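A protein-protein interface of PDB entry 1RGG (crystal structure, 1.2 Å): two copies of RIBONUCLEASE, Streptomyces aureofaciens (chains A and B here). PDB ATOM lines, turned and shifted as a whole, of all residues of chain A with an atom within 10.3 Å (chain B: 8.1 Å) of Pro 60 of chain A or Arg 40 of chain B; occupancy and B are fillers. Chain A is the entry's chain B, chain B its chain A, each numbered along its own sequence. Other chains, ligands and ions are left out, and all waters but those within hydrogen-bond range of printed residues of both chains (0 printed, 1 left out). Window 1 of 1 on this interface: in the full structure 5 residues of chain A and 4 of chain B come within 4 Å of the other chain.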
ATOM      1  N   LEU A  11       8.700  21.411 -13.841  1.00  0.00           N
ATOM      2  CA  LEU A  11       8.744  19.956 -13.765  1.00  0.00           C
ATOM      3  C   LEU A  11       7.699  19.461 -12.788  1.00  0.00           C
ATOM      4  O   LEU A  11       7.149  20.182 -11.945  1.00  0.00           O
ATOM      5  CB  LEU A  11      10.158  19.561 -13.216  1.00  0.00           C
ATOM      6  CG  LEU A  11      11.293  19.806 -14.200  1.00  0.00           C
ATOM      7  CD1 LEU A  11      12.598  19.338 -13.599  1.00  0.00           C
ATOM      8  CD2 LEU A  11      11.029  19.094 -15.514  1.00  0.00           C
ATOM      9  N   PRO A  12       7.395  18.159 -12.845  1.00  0.00           N
ATOM     10  CA  PRO A  12       6.464  17.588 -11.871  1.00  0.00           C
ATOM     11  C   PRO A  12       6.951  17.872 -10.464  1.00  0.00           C
ATOM     12  O   PRO A  12       8.183  17.905 -10.224  1.00  0.00           O
ATOM     13  CB  PRO A  12       6.456  16.100 -12.207  1.00  0.00           C
ATOM     14  CG  PRO A  12       6.904  16.030 -13.590  1.00  0.00           C
ATOM     15  CD  PRO A  12       7.875  17.135 -13.804  1.00  0.00           C
ATOM     16  N   PRO A  13       6.063  17.962  -9.503  1.00  0.00           N
ATOM     17  CA  PRO A  13       6.492  18.294  -8.166  1.00  0.00           C
ATOM     18  C   PRO A  13       7.435  17.281  -7.568  1.00  0.00           C
ATOM     19  O   PRO A  13       8.231  17.579  -6.664  1.00  0.00           O
ATOM     20  CB  PRO A  13       5.198  18.386  -7.362  1.00  0.00           C
ATOM     21  CG  PRO A  13       4.146  17.863  -8.250  1.00  0.00           C
ATOM     22  CD  PRO A  13       4.600  17.949  -9.646  1.00  0.00           C
ATOM     23  N   GLU A  14       7.340  16.027  -7.974  1.00  0.00           N
ATOM     24  CA  GLU A  14       8.206  14.948  -7.437  1.00  0.00           C
ATOM     25  C   GLU A  14       9.645  15.149  -7.782  1.00  0.00           C
ATOM     26  O   GLU A  14      10.538  14.602  -7.119  1.00  0.00           O
ATOM     27  CB  GLU A  14       7.706  13.613  -7.912  1.00  0.00           C
ATOM     28  CG  GLU A  14       6.311  13.241  -7.419  1.00  0.00           C
ATOM     29  CD  GLU A  14       5.176  13.892  -8.100  1.00  0.00           C
ATOM     30  OE1 GLU A  14       5.333  14.371  -9.279  1.00  0.00           O
ATOM     31  OE2 GLU A  14       4.081  13.965  -7.564  1.00  0.00           O
ATOM     32  N   ALA A  15       9.945  15.953  -8.799  1.00  0.00           N
ATOM     33  CA  ALA A  15      11.357  16.278  -9.101  1.00  0.00           C
ATOM     34  C   ALA A  15      11.987  17.068  -8.000  1.00  0.00           C
ATOM     35  O   ALA A  15      13.142  16.876  -7.722  1.00  0.00           O
ATOM     36  CB  ALA A  15      11.468  17.018 -10.433  1.00  0.00           C
ATOM     37  N   ASP A  17      11.102  16.791  -4.812  1.00  0.00           N
ATOM     38  CA  ASP A  17      11.274  15.786  -3.815  1.00  0.00           C
ATOM     39  C   ASP A  17      12.595  15.064  -4.008  1.00  0.00           C
ATOM     40  O   ASP A  17      13.384  14.886  -3.092  1.00  0.00           O
ATOM     41  CB  ASP A  17      10.176  14.763  -3.715  1.00  0.00           C
ATOM     42  CG  ASP A  17       8.816  15.356  -3.387  1.00  0.00           C
ATOM     43  OD1 ASP A  17       8.750  16.428  -2.806  1.00  0.00           O
ATOM     44  OD2 ASP A  17       7.802  14.674  -3.702  1.00  0.00           O
ATOM     45  N   THR A  18      12.852  14.629  -5.234  1.00  0.00           N
ATOM     46  CA  THR A  18      14.090  13.917  -5.530  1.00  0.00           C
ATOM     47  C   THR A  18      15.297  14.772  -5.284  1.00  0.00           C
ATOM     48  O   THR A  18      16.301  14.325  -4.704  1.00  0.00           O
ATOM     49  CB  THR A  18      14.067  13.304  -6.932  1.00  0.00           C
ATOM     50  OG1 THR A  18      12.916  12.501  -7.040  1.00  0.00           O
ATOM     51  CG2 THR A  18      15.307  12.572  -7.239  1.00  0.00           C
ATOM     52  N   TYR A  30      14.021   3.779  -3.329  1.00  0.00           N
ATOM     53  CA  TYR A  30      14.332   2.608  -4.122  1.00  0.00           C
ATOM     54  C   TYR A  30      15.722   2.168  -3.938  1.00  0.00           C
ATOM     55  O   TYR A  30      16.658   3.030  -3.882  1.00  0.00           O
ATOM     56  CB  TYR A  30      14.036   2.858  -5.605  1.00  0.00           C
ATOM     57  CG  TYR A  30      12.548   2.940  -5.880  1.00  0.00           C
ATOM     58  CD1 TYR A  30      11.790   1.767  -5.921  1.00  0.00           C
ATOM     59  CD2 TYR A  30      11.876   4.089  -6.139  1.00  0.00           C
ATOM     60  CE1 TYR A  30      10.456   1.753  -6.173  1.00  0.00           C
ATOM     61  CE2 TYR A  30      10.495   4.115  -6.392  1.00  0.00           C
ATOM     62  CZ  TYR A  30       9.812   2.917  -6.413  1.00  0.00           C
ATOM     63  OH  TYR A  30       8.469   2.914  -6.736  1.00  0.00           O
ATOM     64  N   THR A  56      15.442   8.071  -8.912  1.00  0.00           N
ATOM     65  CA  THR A  56      14.054   8.014  -9.341  1.00  0.00           C
ATOM     66  C   THR A  56      13.330   9.306  -9.029  1.00  0.00           C
ATOM     67  O   THR A  56      13.423   9.830  -7.915  1.00  0.00           O
ATOM     68  CB  THR A  56      13.327   6.863  -8.598  1.00  0.00           C
ATOM     69  OG1 THR A  56      14.058   5.657  -8.710  1.00  0.00           O
ATOM     70  CG2 THR A  56      11.957   6.633  -9.181  1.00  0.00           C
ATOM     71  N   VAL A  57      12.538   9.762  -9.987  1.00  0.00           N
ATOM     72  CA  VAL A  57      11.497  10.761  -9.732  1.00  0.00           C
ATOM     73  C   VAL A  57      10.171   9.943  -9.788  1.00  0.00           C
ATOM     74  O   VAL A  57       9.838   9.379 -10.800  1.00  0.00           O
ATOM     75  CB  VAL A  57      11.475  11.857 -10.797  1.00  0.00           C
ATOM     76  CG1 VAL A  57      10.261  12.758 -10.616  1.00  0.00           C
ATOM     77  CG2 VAL A  57      12.778  12.630 -10.764  1.00  0.00           C
ATOM     78  N   ILE A  58       9.515   9.855  -8.649  1.00  0.00           N
ATOM     79  CA  ILE A  58       8.295   9.002  -8.600  1.00  0.00           C
ATOM     80  C   ILE A  58       7.269   9.574  -9.543  1.00  0.00           C
ATOM     81  O   ILE A  58       7.071  10.794  -9.607  1.00  0.00           O
ATOM     82  CB  ILE A  58       7.772   9.009  -7.107  1.00  0.00           C
ATOM     83  CG1 ILE A  58       8.754   8.096  -6.300  1.00  0.00           C
ATOM     84  CG2 ILE A  58       6.355   8.422  -7.080  1.00  0.00           C
ATOM     85  CD1 ILE A  58       8.503   8.138  -4.849  1.00  0.00           C
ATOM     86  N   THR A  59       6.578   8.682 -10.268  1.00  0.00           N
ATOM     87  CA  THR A  59       5.418   9.049 -11.081  1.00  0.00           C
ATOM     88  C   THR A  59       4.176   8.479 -10.338  1.00  0.00           C
ATOM     89  O   THR A  59       3.935   7.303 -10.298  1.00  0.00           O
ATOM     90  CB  THR A  59       5.509   8.395 -12.455  1.00  0.00           C
ATOM     91  OG1 THR A  59       6.653   8.875 -13.117  1.00  0.00           O
ATOM     92  CG2 THR A  59       4.326   8.802 -13.336  1.00  0.00           C
ATOM     93  N   PRO A  60       3.367   9.398  -9.763  1.00  0.00           N
ATOM     94  CA  PRO A  60       2.144   8.896  -9.103  1.00  0.00           C
ATOM     95  C   PRO A  60       1.280   8.208 -10.130  1.00  0.00           C
ATOM     96  O   PRO A  60       1.173   8.649 -11.294  1.00  0.00           O
ATOM     97  CB  PRO A  60       1.484  10.195  -8.589  1.00  0.00           C
ATOM     98  CG  PRO A  60       2.637  11.149  -8.456  1.00  0.00           C
ATOM     99  CD  PRO A  60       3.516  10.868  -9.676  1.00  0.00           C
ATOM    100  N   GLY A  61       0.644   7.116  -9.735  1.00  0.00           N
ATOM    101  CA  GLY A  61      -0.197   6.357 -10.573  1.00  0.00           C
ATOM    102  C   GLY A  61       0.469   5.260 -11.388  1.00  0.00           C
ATOM    103  O   GLY A  61      -0.190   4.381 -11.884  1.00  0.00           O
ATOM    104  N   ALA A  62       1.803   5.295 -11.482  1.00  0.00           N
ATOM    105  CA  ALA A  62       2.534   4.282 -12.220  1.00  0.00           C
ATOM    106  C   ALA A  62       2.665   3.008 -11.388  1.00  0.00           C
ATOM    107  O   ALA A  62       2.830   3.078 -10.191  1.00  0.00           O
ATOM    108  CB  ALA A  62       3.876   4.776 -12.625  1.00  0.00           C
ATOM    109  N   ARG A  63       2.691   1.853 -12.018  1.00  0.00           N
ATOM    110  CA  ARG A  63       2.861   0.602 -11.313  1.00  0.00           C
ATOM    111  C   ARG A  63       4.304   0.182 -11.132  1.00  0.00           C
ATOM    112  O   ARG A  63       4.585  -0.757 -10.392  1.00  0.00           O
ATOM    113  CB  ARG A  63       2.080  -0.588 -11.859  1.00  0.00           C
ATOM    114  CG  ARG A  63       2.383  -1.121 -13.167  1.00  0.00           C
ATOM    115  CD  ARG A  63       1.875  -2.441 -13.380  1.00  0.00           C
ATOM    116  NE  ARG A  63       2.429  -3.434 -12.699  1.00  0.00           N
ATOM    117  CZ  ARG A  63       3.632  -3.904 -12.499  1.00  0.00           C
ATOM    118  NH1 ARG A  63       4.578  -3.677 -13.355  1.00  0.00           N
ATOM    119  NH2 ARG A  63       3.868  -4.607 -11.463  1.00  0.00           N
ATOM    120  N   THR A  64       5.206   0.847 -11.819  1.00  0.00           N
ATOM    121  CA  THR A  64       6.652   0.605 -11.786  1.00  0.00           C
ATOM    122  C   THR A  64       7.339   1.873 -11.284  1.00  0.00           C
ATOM    123  O   THR A  64       6.694   2.865 -11.031  1.00  0.00           O
ATOM    124  CB  THR A  64       7.160   0.256 -13.179  1.00  0.00           C
ATOM    125  OG1 THR A  64       7.122   1.447 -13.986  1.00  0.00           O
ATOM    126  CG2 THR A  64       6.358  -0.817 -13.857  1.00  0.00           C
ATOM    127  N   ARG A  65       8.655   1.874 -11.273  1.00  0.00           N
ATOM    128  CA  ARG A  65       9.466   3.061 -11.079  1.00  0.00           C
ATOM    129  C   ARG A  65       9.270   4.069 -12.145  1.00  0.00           C
ATOM    130  O   ARG A  65       9.700   5.208 -11.987  1.00  0.00           O
ATOM    131  CB  ARG A  65      10.954   2.705 -10.921  1.00  0.00           C
ATOM    132  CG  ARG A  65      11.392   2.221  -9.609  1.00  0.00           C
ATOM    133  CD  ARG A  65      12.938   2.358  -9.512  1.00  0.00           C
ATOM    134  NE  ARG A  65      13.750   1.999 -10.572  1.00  0.00           N
ATOM    135  CZ  ARG A  65      14.897   2.502 -10.923  1.00  0.00           C
ATOM    136  NH1 ARG A  65      15.315   3.678 -10.477  1.00  0.00           N
ATOM    137  NH2 ARG A  65      15.679   1.849 -11.719  1.00  0.00           N
ATOM    138  N   GLY A  66       8.668   3.733 -13.257  1.00  0.00           N
ATOM    139  CA  GLY A  66       8.391   4.670 -14.330  1.00  0.00           C
ATOM    140  C   GLY A  66       9.624   5.118 -15.082  1.00  0.00           C
ATOM    141  O   GLY A  66      10.637   4.431 -15.063  1.00  0.00           O
ATOM    142  N   THR A  67       9.492   6.235 -15.757  1.00  0.00           N
ATOM    143  CA  THR A  67      10.450   6.718 -16.737  1.00  0.00           C
ATOM    144  C   THR A  67      11.112   8.018 -16.408  1.00  0.00           C
ATOM    145  O   THR A  67      11.870   8.544 -17.211  1.00  0.00           O
ATOM    146  CB  THR A  67       9.777   6.795 -18.105  1.00  0.00           C
ATOM    147  OG1 THR A  67       8.784   7.779 -18.142  1.00  0.00           O
ATOM    148  CG2 THR A  67       9.226   5.455 -18.522  1.00  0.00           C
ATOM    149  N   ARG A  68      10.818   8.578 -15.230  1.00  0.00           N
ATOM    150  CA  ARG A  68      11.341   9.874 -14.842  1.00  0.00           C
ATOM    151  C   ARG A  68      12.528   9.712 -13.903  1.00  0.00           C
ATOM    152  O   ARG A  68      12.450   8.961 -12.928  1.00  0.00           O
ATOM    153  CB  ARG A  68      10.222  10.711 -14.207  1.00  0.00           C
ATOM    154  CG  ARG A  68       9.036  10.885 -15.069  1.00  0.00           C
ATOM    155  CD  ARG A  68       7.904  11.651 -14.444  1.00  0.00           C
ATOM    156  NE  ARG A  68       6.809  11.799 -15.395  1.00  0.00           N
ATOM    157  CZ  ARG A  68       5.663  12.434 -15.189  1.00  0.00           C
ATOM    158  NH1 ARG A  68       5.416  12.921 -14.005  1.00  0.00           N
ATOM    159  NH2 ARG A  68       4.813  12.587 -16.181  1.00  0.00           N
ATOM    160  N   TYR A  81      17.246  16.301 -15.874  1.00  0.00           N
ATOM    161  CA  TYR A  81      15.962  15.593 -15.829  1.00  0.00           C
ATOM    162  C   TYR A  81      15.743  14.852 -17.112  1.00  0.00           C
ATOM    163  O   TYR A  81      15.951  15.388 -18.219  1.00  0.00           O
ATOM    164  CB  TYR A  81      14.828  16.619 -15.650  1.00  0.00           C
ATOM    165  CG  TYR A  81      13.464  16.008 -15.624  1.00  0.00           C
ATOM    166  CD1 TYR A  81      13.001  15.366 -14.484  1.00  0.00           C
ATOM    167  CD2 TYR A  81      12.652  16.017 -16.726  1.00  0.00           C
ATOM    168  CE1 TYR A  81      11.701  14.855 -14.439  1.00  0.00           C
ATOM    169  CE2 TYR A  81      11.408  15.468 -16.684  1.00  0.00           C
ATOM    170  CZ  TYR A  81      10.914  14.882 -15.563  1.00  0.00           C
ATOM    171  OH  TYR A  81       9.659  14.355 -15.478  1.00  0.00           O
ATOM    172  N   PHE B  37      -3.996  -2.009   0.547  1.00  0.00           N
ATOM    173  CA  PHE B  37      -4.016  -0.661   0.033  1.00  0.00           C
ATOM    174  C   PHE B  37      -2.798  -0.473  -0.876  1.00  0.00           C
ATOM    175  O   PHE B  37      -1.698  -0.624  -0.418  1.00  0.00           O
ATOM    176  CB  PHE B  37      -3.987   0.323   1.189  1.00  0.00           C
ATOM    177  CG  PHE B  37      -3.992   1.749   0.752  1.00  0.00           C
ATOM    178  CD1 PHE B  37      -5.121   2.312   0.189  1.00  0.00           C
ATOM    179  CD2 PHE B  37      -2.859   2.518   0.881  1.00  0.00           C
ATOM    180  CE1 PHE B  37      -5.122   3.628  -0.234  1.00  0.00           C
ATOM    181  CE2 PHE B  37      -2.868   3.828   0.468  1.00  0.00           C
ATOM    182  CZ  PHE B  37      -3.995   4.401  -0.085  1.00  0.00           C
ATOM    183  N   GLN B  38      -3.018  -0.166  -2.133  1.00  0.00           N
ATOM    184  CA  GLN B  38      -1.992  -0.138  -3.126  1.00  0.00           C
ATOM    185  C   GLN B  38      -1.084   1.098  -3.044  1.00  0.00           C
ATOM    186  O   GLN B  38      -0.016   1.082  -3.620  1.00  0.00           O
ATOM    187  CB  GLN B  38      -2.599  -0.117  -4.545  1.00  0.00           C
ATOM    188  CG  GLN B  38      -3.179  -1.325  -5.008  1.00  0.00           C
ATOM    189  CD  GLN B  38      -3.437  -1.146  -6.569  1.00  0.00           C
ATOM    190  OE1 GLN B  38      -2.507  -0.676  -7.315  1.00  0.00           O
ATOM    191  NE2 GLN B  38      -4.466  -1.672  -6.928  1.00  0.00           N
ATOM    192  N   ASN B  39      -1.557   2.168  -2.443  1.00  0.00           N
ATOM    193  CA  ASN B  39      -0.783   3.389  -2.421  1.00  0.00           C
ATOM    194  C   ASN B  39      -0.433   3.842  -3.824  1.00  0.00           C
ATOM    195  O   ASN B  39       0.673   4.303  -4.078  1.00  0.00           O
ATOM    196  CB  ASN B  39       0.474   3.270  -1.557  1.00  0.00           C
ATOM    197  CG  ASN B  39       1.144   4.545  -1.233  1.00  0.00           C
ATOM    198  OD1 ASN B  39       0.500   5.579  -1.073  1.00  0.00           O
ATOM    199  ND2 ASN B  39       2.485   4.499  -1.094  1.00  0.00           N
ATOM    200  N   ARG B  40      -1.413   3.770  -4.718  1.00  0.00           N
ATOM    201  CA  ARG B  40      -1.168   4.031  -6.136  1.00  0.00           C
ATOM    202  C   ARG B  40      -0.703   5.451  -6.372  1.00  0.00           C
ATOM    203  O   ARG B  40       0.052   5.703  -7.333  1.00  0.00           O
ATOM    204  CB  ARG B  40      -2.400   3.682  -6.930  1.00  0.00           C
ATOM    205  CG  ARG B  40      -2.445   3.840  -8.395  1.00  0.00           C
ATOM    206  CD  ARG B  40      -2.916   2.553  -9.068  1.00  0.00           C
ATOM    207  NE  ARG B  40      -2.369   2.416 -10.393  1.00  0.00           N
ATOM    208  CZ  ARG B  40      -1.960   1.268 -10.914  1.00  0.00           C
ATOM    209  NH1 ARG B  40      -2.244   0.102 -10.376  1.00  0.00           N
ATOM    210  NH2 ARG B  40      -1.340   1.291 -12.073  1.00  0.00           N
ATOM    211  N   GLU B  41      -1.198   6.408  -5.621  1.00  0.00           N
ATOM    212  CA  GLU B  41      -0.902   7.809  -5.821  1.00  0.00           C
ATOM    213  C   GLU B  41       0.364   8.239  -5.089  1.00  0.00           C
ATOM    214  O   GLU B  41       0.744   9.401  -5.145  1.00  0.00           O
ATOM    215  CB  GLU B  41      -2.088   8.720  -5.413  1.00  0.00           C
ATOM    216  CG  GLU B  41      -3.311   8.536  -6.208  1.00  0.00           C
ATOM    217  CD  GLU B  41      -4.062   7.294  -6.245  1.00  0.00           C
ATOM    218  OE1 GLU B  41      -4.155   6.553  -5.217  1.00  0.00           O
ATOM    219  OE2 GLU B  41      -4.431   6.903  -7.377  1.00  0.00           O
ATOM    220  N   SER B  42       1.054   7.325  -4.396  1.00  0.00           N
ATOM    221  CA  SER B  42       2.284   7.626  -3.725  1.00  0.00           C
ATOM    222  C   SER B  42       2.199   8.696  -2.680  1.00  0.00           C
ATOM    223  O   SER B  42       3.126   9.417  -2.392  1.00  0.00           O
ATOM    224  CB  SER B  42       3.368   7.998  -4.803  1.00  0.00           C
ATOM    225  OG  SER B  42       4.612   7.796  -4.205  1.00  0.00           O
ATOM    226  N   VAL B  43       1.066   8.726  -1.970  1.00  0.00           N
ATOM    227  CA  VAL B  43       0.901   9.677  -0.860  1.00  0.00           C
ATOM    228  C   VAL B  43       1.660   9.197   0.371  1.00  0.00           C
ATOM    229  O   VAL B  43       2.283   9.991   1.058  1.00  0.00           O
ATOM    230  CB  VAL B  43      -0.557   9.929  -0.545  1.00  0.00           C
ATOM    231  CG1 VAL B  43      -0.665  10.954   0.594  1.00  0.00           C
ATOM    232  CG2 VAL B  43      -1.229  10.631  -1.794  1.00  0.00           C
ATOM    233  N   LEU B  44       1.636   7.891   0.648  1.00  0.00           N
ATOM    234  CA  LEU B  44       2.373   7.290   1.718  1.00  0.00           C
ATOM    235  C   LEU B  44       3.742   6.886   1.227  1.00  0.00           C
ATOM    236  O   LEU B  44       3.952   6.761   0.009  1.00  0.00           O
ATOM    237  CB  LEU B  44       1.640   6.069   2.287  1.00  0.00           C
ATOM    238  CG  LEU B  44       0.270   6.402   2.899  1.00  0.00           C
ATOM    239  CD1 LEU B  44      -0.373   5.123   3.400  1.00  0.00           C
ATOM    240  CD2 LEU B  44       0.390   7.433   4.004  1.00  0.00           C
ATOM    241  N   TYR B  52       0.777  -2.235   3.057  1.00  0.00           N
ATOM    242  CA  TYR B  52      -0.325  -1.468   3.579  1.00  0.00           C
ATOM    243  C   TYR B  52      -1.641  -2.207   3.439  1.00  0.00           C
ATOM    244  O   TYR B  52      -1.893  -2.836   2.424  1.00  0.00           O
ATOM    245  CB  TYR B  52      -0.457  -0.130   2.852  1.00  0.00           C
ATOM    246  CG  TYR B  52       0.728   0.792   2.970  1.00  0.00           C
ATOM    247  CD1 TYR B  52       1.082   1.429   4.154  1.00  0.00           C
ATOM    248  CD2 TYR B  52       1.501   1.085   1.862  1.00  0.00           C
ATOM    249  CE1 TYR B  52       2.117   2.292   4.228  1.00  0.00           C
ATOM    250  CE2 TYR B  52       2.571   1.958   1.922  1.00  0.00           C
ATOM    251  CZ  TYR B  52       2.883   2.565   3.096  1.00  0.00           C
ATOM    252  OH  TYR B  52       3.908   3.477   3.241  1.00  0.00           O
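OE1 of Gln 38 of chain B sits at hydrogen-bond distance from NH1 of Arg 40 of chain B, at 3.2 Å.
Of the printed residues of chain B, Ile 58 of chain A touches Ser 42. Of the printed residues of chain B, Pro 60 of chain A touches Arg 40 (3.95 Å) and Glu 41 (3.6 Å). Gly 61 of chain A touches one residue of chain B. Of the printed residues of chain B, Arg 63 of chain A touches Arg 40. Of the printed residues of chain A, Glu 41 of chain B touches Pro 60. Printed residues of chain A within 4 Å of Ser 42 of chain B: Ile 58.
CG2 of Ile 58 of chain A touches OG of Ser 42 of chain B, at 3.4 Å. Arg 40 of chain B touches Pro 60 of chain A. Glu 41 of chain B touches Pro 60 of chain A (O to CB, 3.6 Å). CB of Arg 63 of chain A touches NH2 of Arg 40 of chain B, 3.9 Å away.
No position is printed for both chains.
O of Arg 40 of chain B lies within hydrogen-bond range of N of Gly 61 of chain A, at 2.8 Å.
Printed residues of chain B that touch a printed residue of chain A: Arg 40, Glu 41 and Ser 42. Along chain B the printed residues that touch a printed residue of chain A span positions 40 to 42. Hydrophobic or aromatic side chains of chain A within 4 Å of the printed part of chain B: Ile 58 and Pro 60. Among the printed residues, 5 pairs touch across the chains. Among the printed residues, no Asp or Glu carboxylate lies within 4 Å of a Lys or Arg side-chain nitrogen of the other chain.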
